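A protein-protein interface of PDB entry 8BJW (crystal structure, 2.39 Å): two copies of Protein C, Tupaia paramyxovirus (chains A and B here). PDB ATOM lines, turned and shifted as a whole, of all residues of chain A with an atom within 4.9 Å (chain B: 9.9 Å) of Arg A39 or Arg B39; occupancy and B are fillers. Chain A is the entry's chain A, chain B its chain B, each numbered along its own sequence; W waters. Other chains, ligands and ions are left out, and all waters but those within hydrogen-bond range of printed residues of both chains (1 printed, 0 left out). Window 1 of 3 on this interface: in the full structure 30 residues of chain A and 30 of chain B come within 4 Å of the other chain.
OH of Tyr A43 sits close to N of Ser B29 (3.3 Å).
O of Thr B27 sits at hydrogen-bond distance from OH of Tyr A43, at 2.6 Å.
The side-chain carboxylate of Asp A40 lies within salt-bridge range of the guanidinium group of Arg B36, 3.2 Å away.
The guanidinium group (NH2) of Arg A36 lies close to the guanidinium group (NH1) of Arg B36 (3.4 Å).
OD1 of Asp B40 is in salt-bridge range of NE of Arg A36 (2.8 Å).
NE of Arg A39 lies close to NE of Arg B39, 2.9 Å away.
ND2 of Asn B44 sits at hydrogen-bond distance from O of Asp B40, 2.9 Å away.
NH1 of Arg B39 sits close to NE2 of Gln B35, 3.4 Å away.
Among the printed residues, pairs that only touch across the chains: Asn A32 with Tyr B43 (3.4 Å) and Tyr A43 with Asn B32 (3.3 Å).
Of the printed residues of chain B, Arg A39 touches Arg B39 (2.9 Å).
Arg B39 touches one residue of chain A.
Of chain B, only Arg B36 comes within 4 Å of Asp A40.
Of the printed residues of chain A, Ser B29 touches Tyr A43 (3.3 Å).
Of the printed residues of chain A, Asn B32 touches Tyr A43 (3.3 Å).
Printed residues of chain A within 4 Å of Thr B27: Tyr A43 (2.6 Å).
Of the printed residues of chain B, Asn A32 touches Tyr B43.
Of the printed residues of chain B, Arg A36 touches Arg B36 (3.4 Å) and Asp B40 (2.8 Å).
Glu B46 touches none of the printed residues of chain A.
Asn B38 touches none of the printed residues of chain A.
The nearest residue of chain A that does not touch Arg B39 is Asp A40 (4.6 Å).
Of the 20 printed residues of chain B, 7 touch a printed residue of chain A.
Hydrophobic or aromatic side chains of chain A that line the printed part of chain B: Tyr A43.
Along chain A the printed residues that touch a printed residue of chain B span positions 32 to 43.
Among the printed residues, 8 pairs touch across the chains.
Asn A32 touches Tyr B43, and with the chains exchanged Tyr A43 touches Asn B32.
Arg A36 touches its own counterpart, Arg B36.
Arg A36 touches Asp B40, and with the chains exchanged Asp A40 touches Arg B36.
Arg B39 touches its own counterpart, Arg A39.
10 positions are printed for both chains.
Water W1 bridges NH2 of Arg A39 and NE of Arg B39.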
ATOM      1  N   ASN A  32     -23.964  21.885  -9.214  1.00  0.00           N
ATOM      2  CA  ASN A  32     -24.305  22.575  -7.943  1.00  0.00           C
ATOM      3  C   ASN A  32     -23.449  21.976  -6.826  1.00  0.00           C
ATOM      4  O   ASN A  32     -23.115  22.710  -5.868  1.00  0.00           O
ATOM      5  CB  ASN A  32     -25.811  22.508  -7.658  1.00  0.00           C
ATOM      6  CG  ASN A  32     -26.208  22.834  -6.235  1.00  0.00           C
ATOM      7  OD1 ASN A  32     -26.356  21.911  -5.420  1.00  0.00           O
ATOM      8  ND2 ASN A  32     -26.255  24.127  -5.919  1.00  0.00           N
ATOM      9  N   GLN A  35     -20.105  23.787  -7.297  1.00  0.00           N
ATOM     10  CA  GLN A  35     -20.232  25.219  -6.886  1.00  0.00           C
ATOM     11  C   GLN A  35     -20.268  25.314  -5.357  1.00  0.00           C
ATOM     12  O   GLN A  35     -19.585  26.185  -4.779  1.00  0.00           O
ATOM     13  CB  GLN A  35     -21.468  25.864  -7.489  1.00  0.00           C
ATOM     14  CG  GLN A  35     -21.308  26.194  -8.954  1.00  0.00           C
ATOM     15  CD  GLN A  35     -22.579  26.797  -9.517  1.00  0.00           C
ATOM     16  OE1 GLN A  35     -23.521  27.162  -8.787  1.00  0.00           O
ATOM     17  NE2 GLN A  35     -22.627  26.883 -10.845  1.00  0.00           N
ATOM     18  N   ARG A  36     -21.003  24.414  -4.723  1.00  0.00           N
ATOM     19  CA  ARG A  36     -21.234  24.437  -3.262  1.00  0.00           C
ATOM     20  C   ARG A  36     -19.918  24.098  -2.572  1.00  0.00           C
ATOM     21  O   ARG A  36     -19.560  24.732  -1.555  1.00  0.00           O
ATOM     22  CB  ARG A  36     -22.357  23.423  -3.018  1.00  0.00           C
ATOM     23  CG  ARG A  36     -22.646  23.059  -1.588  1.00  0.00           C
ATOM     24  CD  ARG A  36     -23.873  22.143  -1.613  1.00  0.00           C
ATOM     25  NE  ARG A  36     -24.124  21.970  -0.197  1.00  0.00           N
ATOM     26  CZ  ARG A  36     -23.538  21.056   0.567  1.00  0.00           C
ATOM     27  NH1 ARG A  36     -22.718  20.180   0.007  1.00  0.00           N
ATOM     28  NH2 ARG A  36     -23.787  21.039   1.867  1.00  0.00           N
ATOM     29  N   ASN A  37     -19.199  23.142  -3.131  1.00  0.00           N
ATOM     30  CA  ASN A  37     -17.898  22.698  -2.597  1.00  0.00           C
ATOM     31  C   ASN A  37     -16.869  23.836  -2.772  1.00  0.00           C
ATOM     32  O   ASN A  37     -16.193  24.131  -1.802  1.00  0.00           O
ATOM     33  CB  ASN A  37     -17.527  21.389  -3.268  1.00  0.00           C
ATOM     34  CG  ASN A  37     -16.313  20.810  -2.632  1.00  0.00           C
ATOM     35  OD1 ASN A  37     -15.252  20.907  -3.196  1.00  0.00           O
ATOM     36  ND2 ASN A  37     -16.477  20.263  -1.449  1.00  0.00           N
ATOM     37  N   ASN A  38     -16.848  24.523  -3.908  1.00  0.00           N
ATOM     38  CA  ASN A  38     -15.989  25.715  -4.123  1.00  0.00           C
ATOM     39  C   ASN A  38     -16.273  26.775  -3.061  1.00  0.00           C
ATOM     40  O   ASN A  38     -15.283  27.258  -2.449  1.00  0.00           O
ATOM     41  CB  ASN A  38     -16.181  26.323  -5.504  1.00  0.00           C
ATOM     42  CG  ASN A  38     -15.603  25.465  -6.600  1.00  0.00           C
ATOM     43  OD1 ASN A  38     -14.877  24.522  -6.347  1.00  0.00           O
ATOM     44  ND2 ASN A  38     -15.890  25.809  -7.830  1.00  0.00           N
ATOM     45  N   ARG A  39     -17.548  27.109  -2.809  1.00  0.00           N
ATOM     46  CA  ARG A  39     -17.887  28.178  -1.841  1.00  0.00           C
ATOM     47  C   ARG A  39     -17.330  27.790  -0.466  1.00  0.00           C
ATOM     48  O   ARG A  39     -16.817  28.699   0.260  1.00  0.00           O
ATOM     49  CB  ARG A  39     -19.390  28.430  -1.734  1.00  0.00           C
ATOM     50  CG  ARG A  39     -20.038  29.050  -2.954  1.00  0.00           C
ATOM     51  CD  ARG A  39     -21.451  29.545  -2.639  1.00  0.00           C
ATOM     52  NE  ARG A  39     -22.428  28.502  -2.338  1.00  0.00           N
ATOM     53  CZ  ARG A  39     -23.162  27.831  -3.233  1.00  0.00           C
ATOM     54  NH1 ARG A  39     -23.034  28.049  -4.531  1.00  0.00           N
ATOM     55  NH2 ARG A  39     -24.037  26.920  -2.828  1.00  0.00           N
ATOM     56  N   ASP A  40     -17.470  26.523  -0.098  1.00  0.00           N
ATOM     57  CA  ASP A  40     -17.141  26.025   1.255  1.00  0.00           C
ATOM     58  C   ASP A  40     -15.616  26.021   1.409  1.00  0.00           C
ATOM     59  O   ASP A  40     -15.160  26.455   2.458  1.00  0.00           O
ATOM     60  CB  ASP A  40     -17.741  24.643   1.548  1.00  0.00           C
ATOM     61  CG  ASP A  40     -19.287  24.621   1.622  1.00  0.00           C
ATOM     62  OD1 ASP A  40     -19.950  25.706   1.582  1.00  0.00           O
ATOM     63  OD2 ASP A  40     -19.871  23.497   1.694  1.00  0.00           O
ATOM     64  N   LEU A  41     -14.876  25.526   0.407  1.00  0.00           N
ATOM     65  CA  LEU A  41     -13.395  25.572   0.346  1.00  0.00           C
ATOM     66  C   LEU A  41     -12.914  27.020   0.431  1.00  0.00           C
ATOM     67  O   LEU A  41     -12.046  27.286   1.299  1.00  0.00           O
ATOM     68  CB  LEU A  41     -12.927  24.947  -0.974  1.00  0.00           C
ATOM     69  CG  LEU A  41     -12.795  23.431  -1.048  1.00  0.00           C
ATOM     70  CD1 LEU A  41     -11.626  23.087  -1.976  1.00  0.00           C
ATOM     71  CD2 LEU A  41     -12.590  22.804   0.332  1.00  0.00           C
ATOM     72  N   ASP A  42     -13.500  27.925  -0.362  1.00  0.00           N
ATOM     73  CA  ASP A  42     -13.088  29.357  -0.370  1.00  0.00           C
ATOM     74  C   ASP A  42     -13.289  29.909   1.041  1.00  0.00           C
ATOM     75  O   ASP A  42     -12.371  30.542   1.578  1.00  0.00           O
ATOM     76  CB  ASP A  42     -13.778  30.161  -1.480  1.00  0.00           C
ATOM     77  CG  ASP A  42     -13.483  29.657  -2.893  1.00  0.00           C
ATOM     78  OD1 ASP A  42     -12.523  28.830  -3.065  1.00  0.00           O
ATOM     79  OD2 ASP A  42     -14.199  30.098  -3.843  1.00  0.00           O
ATOM     80  N   TYR A  43     -14.420  29.617   1.665  1.00  0.00           N
ATOM     81  CA  TYR A  43     -14.712  30.153   3.005  1.00  0.00           C
ATOM     82  C   TYR A  43     -13.668  29.617   3.990  1.00  0.00           C
ATOM     83  O   TYR A  43     -13.095  30.405   4.768  1.00  0.00           O
ATOM     84  CB  TYR A  43     -16.120  29.799   3.484  1.00  0.00           C
ATOM     85  CG  TYR A  43     -16.377  30.391   4.844  1.00  0.00           C
ATOM     86  CD1 TYR A  43     -16.762  31.718   4.979  1.00  0.00           C
ATOM     87  CD2 TYR A  43     -16.202  29.644   5.994  1.00  0.00           C
ATOM     88  CE1 TYR A  43     -16.959  32.282   6.223  1.00  0.00           C
ATOM     89  CE2 TYR A  43     -16.386  30.199   7.248  1.00  0.00           C
ATOM     90  CZ  TYR A  43     -16.743  31.530   7.362  1.00  0.00           C
ATOM     91  OH  TYR A  43     -16.934  32.117   8.577  1.00  0.00           O
ATOM     92  N   THR B  27     -17.795  36.837   6.993  1.00  0.00           N
ATOM     93  CA  THR B  27     -18.944  36.344   7.799  1.00  0.00           C
ATOM     94  C   THR B  27     -18.345  35.469   8.911  1.00  0.00           C
ATOM     95  O   THR B  27     -17.425  34.673   8.625  1.00  0.00           O
ATOM     96  CB  THR B  27     -19.970  35.683   6.861  1.00  0.00           C
ATOM     97  OG1 THR B  27     -20.443  36.737   6.018  1.00  0.00           O
ATOM     98  CG2 THR B  27     -21.157  35.032   7.529  1.00  0.00           C
ATOM     99  N   SER B  29     -18.306  32.312  11.576  1.00  0.00           N
ATOM    100  CA  SER B  29     -18.389  30.879  11.243  1.00  0.00           C
ATOM    101  C   SER B  29     -19.863  30.418  11.345  1.00  0.00           C
ATOM    102  O   SER B  29     -20.368  29.747  10.420  1.00  0.00           O
ATOM    103  CB  SER B  29     -17.473  30.097  12.123  1.00  0.00           C
ATOM    104  OG  SER B  29     -17.054  28.935  11.439  1.00  0.00           O
ATOM    105  N   ALA B  31     -22.696  32.369  11.319  1.00  0.00           N
ATOM    106  CA  ALA B  31     -23.462  33.094  10.289  1.00  0.00           C
ATOM    107  C   ALA B  31     -23.287  32.386   8.949  1.00  0.00           C
ATOM    108  O   ALA B  31     -24.267  32.321   8.205  1.00  0.00           O
ATOM    109  CB  ALA B  31     -23.027  34.539  10.193  1.00  0.00           C
ATOM    110  N   ASN B  32     -22.086  31.871   8.655  1.00  0.00           N
ATOM    111  CA  ASN B  32     -21.778  31.216   7.361  1.00  0.00           C
ATOM    112  C   ASN B  32     -22.438  29.835   7.329  1.00  0.00           C
ATOM    113  O   ASN B  32     -22.836  29.378   6.248  1.00  0.00           O
ATOM    114  CB  ASN B  32     -20.273  31.141   7.103  1.00  0.00           C
ATOM    115  CG  ASN B  32     -19.923  30.350   5.859  1.00  0.00           C
ATOM    116  OD1 ASN B  32     -19.492  29.210   5.940  1.00  0.00           O
ATOM    117  ND2 ASN B  32     -20.136  30.911   4.695  1.00  0.00           N
ATOM    118  N   LEU B  33     -22.513  29.168   8.474  1.00  0.00           N
ATOM    119  CA  LEU B  33     -23.194  27.860   8.595  1.00  0.00           C
ATOM    120  C   LEU B  33     -24.677  28.074   8.268  1.00  0.00           C
ATOM    121  O   LEU B  33     -25.206  27.306   7.485  1.00  0.00           O
ATOM    122  CB  LEU B  33     -22.976  27.339  10.016  1.00  0.00           C
ATOM    123  CG  LEU B  33     -23.492  25.943  10.330  1.00  0.00           C
ATOM    124  CD1 LEU B  33     -22.882  24.930   9.386  1.00  0.00           C
ATOM    125  CD2 LEU B  33     -23.185  25.600  11.779  1.00  0.00           C
ATOM    126  N   VAL B  34     -25.298  29.124   8.808  1.00  0.00           N
ATOM    127  CA  VAL B  34     -26.718  29.466   8.519  1.00  0.00           C
ATOM    128  C   VAL B  34     -26.880  29.725   7.018  1.00  0.00           C
ATOM    129  O   VAL B  34     -27.714  29.055   6.376  1.00  0.00           O
ATOM    130  CB  VAL B  34     -27.174  30.672   9.366  1.00  0.00           C
ATOM    131  CG1 VAL B  34     -28.514  31.236   8.909  1.00  0.00           C
ATOM    132  CG2 VAL B  34     -27.189  30.317  10.835  1.00  0.00           C
ATOM    133  N   GLN B  35     -26.089  30.641   6.464  1.00  0.00           N
ATOM    134  CA  GLN B  35     -26.200  31.062   5.045  1.00  0.00           C
ATOM    135  C   GLN B  35     -26.078  29.825   4.139  1.00  0.00           C
ATOM    136  O   GLN B  35     -26.860  29.684   3.188  1.00  0.00           O
ATOM    137  CB  GLN B  35     -25.146  32.110   4.731  1.00  0.00           C
ATOM    138  CG  GLN B  35     -25.461  32.943   3.505  1.00  0.00           C
ATOM    139  CD  GLN B  35     -24.414  34.012   3.296  1.00  0.00           C
ATOM    140  OE1 GLN B  35     -23.701  34.396   4.227  1.00  0.00           O
ATOM    141  NE2 GLN B  35     -24.297  34.483   2.058  1.00  0.00           N
ATOM    142  N   ARG B  36     -25.146  28.949   4.456  1.00  0.00           N
ATOM    143  CA  ARG B  36     -24.833  27.762   3.640  1.00  0.00           C
ATOM    144  C   ARG B  36     -26.019  26.796   3.715  1.00  0.00           C
ATOM    145  O   ARG B  36     -26.428  26.209   2.702  1.00  0.00           O
ATOM    146  CB  ARG B  36     -23.529  27.195   4.197  1.00  0.00           C
ATOM    147  CG  ARG B  36     -23.079  25.898   3.560  1.00  0.00           C
ATOM    148  CD  ARG B  36     -21.597  25.681   3.892  1.00  0.00           C
ATOM    149  NE  ARG B  36     -21.455  24.868   5.081  1.00  0.00           N
ATOM    150  CZ  ARG B  36     -21.674  23.559   5.118  1.00  0.00           C
ATOM    151  NH1 ARG B  36     -21.932  22.879   4.004  1.00  0.00           N
ATOM    152  NH2 ARG B  36     -21.568  22.931   6.278  1.00  0.00           N
ATOM    153  N   ASN B  37     -26.588  26.670   4.892  1.00  0.00           N
ATOM    154  CA  ASN B  37     -27.759  25.809   5.140  1.00  0.00           C
ATOM    155  C   ASN B  37     -28.994  26.369   4.405  1.00  0.00           C
ATOM    156  O   ASN B  37     -29.644  25.584   3.721  1.00  0.00           O
ATOM    157  CB  ASN B  37     -27.913  25.652   6.640  1.00  0.00           C
ATOM    158  CG  ASN B  37     -28.956  24.640   6.947  1.00  0.00           C
ATOM    159  OD1 ASN B  37     -30.067  25.019   7.271  1.00  0.00           O
ATOM    160  ND2 ASN B  37     -28.601  23.386   6.772  1.00  0.00           N
ATOM    161  N   ASN B  38     -29.221  27.688   4.442  1.00  0.00           N
ATOM    162  CA  ASN B  38     -30.275  28.350   3.656  1.00  0.00           C
ATOM    163  C   ASN B  38     -30.108  28.042   2.164  1.00  0.00           C
ATOM    164  O   ASN B  38     -31.109  27.653   1.548  1.00  0.00           O
ATOM    165  CB  ASN B  38     -30.300  29.858   3.864  1.00  0.00           C
ATOM    166  CG  ASN B  38     -30.856  30.225   5.220  1.00  0.00           C
ATOM    167  OD1 ASN B  38     -31.400  29.388   5.920  1.00  0.00           O
ATOM    168  ND2 ASN B  38     -30.741  31.481   5.611  1.00  0.00           N
ATOM    169  N   ARG B  39     -28.902  28.187   1.607  1.00  0.00           N
ATOM    170  CA  ARG B  39     -28.680  27.978   0.155  1.00  0.00           C
ATOM    171  C   ARG B  39     -29.045  26.544  -0.192  1.00  0.00           C
ATOM    172  O   ARG B  39     -29.631  26.358  -1.290  1.00  0.00           O
ATOM    173  CB  ARG B  39     -27.239  28.260  -0.279  1.00  0.00           C
ATOM    174  CG  ARG B  39     -26.880  29.741  -0.278  1.00  0.00           C
ATOM    175  CD  ARG B  39     -25.563  29.987  -1.027  1.00  0.00           C
ATOM    176  NE  ARG B  39     -24.377  29.425  -0.370  1.00  0.00           N
ATOM    177  CZ  ARG B  39     -23.659  30.021   0.592  1.00  0.00           C
ATOM    178  NH1 ARG B  39     -23.972  31.231   1.027  1.00  0.00           N
ATOM    179  NH2 ARG B  39     -22.607  29.407   1.107  1.00  0.00           N
ATOM    180  N   ASP B  40     -28.684  25.586   0.664  1.00  0.00           N
ATOM    181  CA  ASP B  40     -28.869  24.139   0.387  1.00  0.00           C
ATOM    182  C   ASP B  40     -30.372  23.817   0.415  1.00  0.00           C
ATOM    183  O   ASP B  40     -30.833  23.112  -0.488  1.00  0.00           O
ATOM    184  CB  ASP B  40     -28.120  23.246   1.376  1.00  0.00           C
ATOM    185  CG  ASP B  40     -26.595  23.320   1.340  1.00  0.00           C
ATOM    186  OD1 ASP B  40     -26.023  23.898   0.352  1.00  0.00           O
ATOM    187  OD2 ASP B  40     -25.975  22.787   2.316  1.00  0.00           O
ATOM    188  N   LEU B  41     -31.083  24.306   1.437  1.00  0.00           N
ATOM    189  CA  LEU B  41     -32.552  24.171   1.586  1.00  0.00           C
ATOM    190  C   LEU B  41     -33.244  24.808   0.363  1.00  0.00           C
ATOM    191  O   LEU B  41     -34.096  24.131  -0.268  1.00  0.00           O
ATOM    192  CB  LEU B  41     -32.951  24.846   2.891  1.00  0.00           C
ATOM    193  CG  LEU B  41     -34.376  24.641   3.374  1.00  0.00           C
ATOM    194  CD1 LEU B  41     -34.448  24.847   4.867  1.00  0.00           C
ATOM    195  CD2 LEU B  41     -35.304  25.615   2.690  1.00  0.00           C
ATOM    196  N   ASP B  42     -32.838  26.026  -0.011  1.00  0.00           N
ATOM    197  CA  ASP B  42     -33.446  26.756  -1.143  1.00  0.00           C
ATOM    198  C   ASP B  42     -33.233  25.929  -2.407  1.00  0.00           C
ATOM    199  O   ASP B  42     -34.171  25.747  -3.149  1.00  0.00           O
ATOM    200  CB  ASP B  42     -32.917  28.198  -1.220  1.00  0.00           C
ATOM    201  CG  ASP B  42     -33.294  29.056   0.000  1.00  0.00           C
ATOM    202  OD1 ASP B  42     -34.104  28.597   0.893  1.00  0.00           O
ATOM    203  OD2 ASP B  42     -32.795  30.185   0.059  1.00  0.00           O
ATOM    204  N   TYR B  43     -32.049  25.384  -2.619  1.00  0.00           N
ATOM    205  CA  TYR B  43     -31.738  24.609  -3.839  1.00  0.00           C
ATOM    206  C   TYR B  43     -32.625  23.367  -3.850  1.00  0.00           C
ATOM    207  O   TYR B  43     -33.261  23.090  -4.903  1.00  0.00           O
ATOM    208  CB  TYR B  43     -30.269  24.191  -3.895  1.00  0.00           C
ATOM    209  CG  TYR B  43     -29.954  23.380  -5.112  1.00  0.00           C
ATOM    210  CD1 TYR B  43     -29.664  24.016  -6.311  1.00  0.00           C
ATOM    211  CD2 TYR B  43     -29.955  22.010  -5.086  1.00  0.00           C
ATOM    212  CE1 TYR B  43     -29.365  23.301  -7.462  1.00  0.00           C
ATOM    213  CE2 TYR B  43     -29.687  21.274  -6.230  1.00  0.00           C
ATOM    214  CZ  TYR B  43     -29.403  21.923  -7.425  1.00  0.00           C
ATOM    215  OH  TYR B  43     -29.146  21.177  -8.546  1.00  0.00           O
ATOM    216  N   ASN B  44     -32.680  22.622  -2.736  1.00  0.00           N
ATOM    217  CA  ASN B  44     -33.444  21.344  -2.687  1.00  0.00           C
ATOM    218  C   ASN B  44     -34.949  21.624  -2.816  1.00  0.00           C
ATOM    219  O   ASN B  44     -35.635  20.850  -3.492  1.00  0.00           O
ATOM    220  CB  ASN B  44     -33.143  20.521  -1.436  1.00  0.00           C
ATOM    221  CG  ASN B  44     -31.670  20.126  -1.369  1.00  0.00           C
ATOM    222  OD1 ASN B  44     -31.043  19.831  -2.378  1.00  0.00           O
ATOM    223  ND2 ASN B  44     -31.053  20.206  -0.206  1.00  0.00           N
ATOM    224  N   LEU B  45     -35.445  22.698  -2.198  1.00  0.00           N
ATOM    225  CA  LEU B  45     -36.866  23.136  -2.329  1.00  0.00           C
ATOM    226  C   LEU B  45     -37.187  23.419  -3.800  1.00  0.00           C
ATOM    227  O   LEU B  45     -38.208  22.900  -4.292  1.00  0.00           O
ATOM    228  CB  LEU B  45     -37.091  24.373  -1.475  1.00  0.00           C
ATOM    229  CG  LEU B  45     -38.502  24.918  -1.480  1.00  0.00           C
ATOM    230  CD1 LEU B  45     -39.449  23.833  -1.029  1.00  0.00           C
ATOM    231  CD2 LEU B  45     -38.629  26.108  -0.564  1.00  0.00           C
ATOM    232  N   GLU B  46     -36.338  24.143  -4.510  1.00  0.00           N
ATOM    233  CA  GLU B  46     -36.603  24.504  -5.919  1.00  0.00           C
ATOM    234  C   GLU B  46     -36.621  23.226  -6.778  1.00  0.00           C
ATOM    235  O   GLU B  46     -37.486  23.137  -7.669  1.00  0.00           O
ATOM    236  CB  GLU B  46     -35.639  25.593  -6.404  1.00  0.00           C
ATOM    237  CG  GLU B  46     -35.819  25.926  -7.861  1.00  0.00           C
ATOM    238  CD  GLU B  46     -37.099  26.631  -8.291  1.00  0.00           C
ATOM    239  OE1 GLU B  46     -37.973  26.909  -7.447  1.00  0.00           O
ATOM    240  OE2 GLU B  46     -37.216  26.934  -9.516  1.00  0.00           O
ATOM    241  N   GLN B  47     -35.787  22.225  -6.511  1.00  0.00           N
ATOM    242  CA  GLN B  47     -35.843  20.952  -7.278  1.00  0.00           C
ATOM    243  C   GLN B  47     -37.185  20.251  -7.030  1.00  0.00           C
ATOM    244  O   GLN B  47     -37.767  19.695  -7.976  1.00  0.00           O
ATOM    245  CB  GLN B  47     -34.742  19.962  -6.880  1.00  0.00           C
ATOM    246  CG  GLN B  47     -33.325  20.324  -7.285  1.00  0.00           C
ATOM    247  CD  GLN B  47     -32.410  19.126  -7.105  1.00  0.00           C
ATOM    248  OE1 GLN B  47     -32.315  18.539  -6.013  1.00  0.00           O
ATOM    249  NE2 GLN B  47     -31.743  18.713  -8.175  1.00  0.00           N
ATOM    250  N   LEU B  83     -38.820  18.382   2.985  1.00  0.00           N
ATOM    251  CA  LEU B  83     -39.210  19.682   2.366  1.00  0.00           C
ATOM    252  C   LEU B  83     -40.507  19.610   1.562  1.00  0.00           C
ATOM    253  O   LEU B  83     -40.857  20.622   0.823  1.00  0.00           O
ATOM    254  CB  LEU B  83     -38.067  20.085   1.426  1.00  0.00           C
ATOM    255  CG  LEU B  83     -36.803  20.586   2.109  1.00  0.00           C
ATOM    256  CD1 LEU B  83     -35.764  20.898   1.067  1.00  0.00           C
ATOM    257  CD2 LEU B  83     -37.077  21.804   2.959  1.00  0.00           C
HETATM  258  O   HOH W   1     -23.447  26.412   0.015  1.00  0.00           O
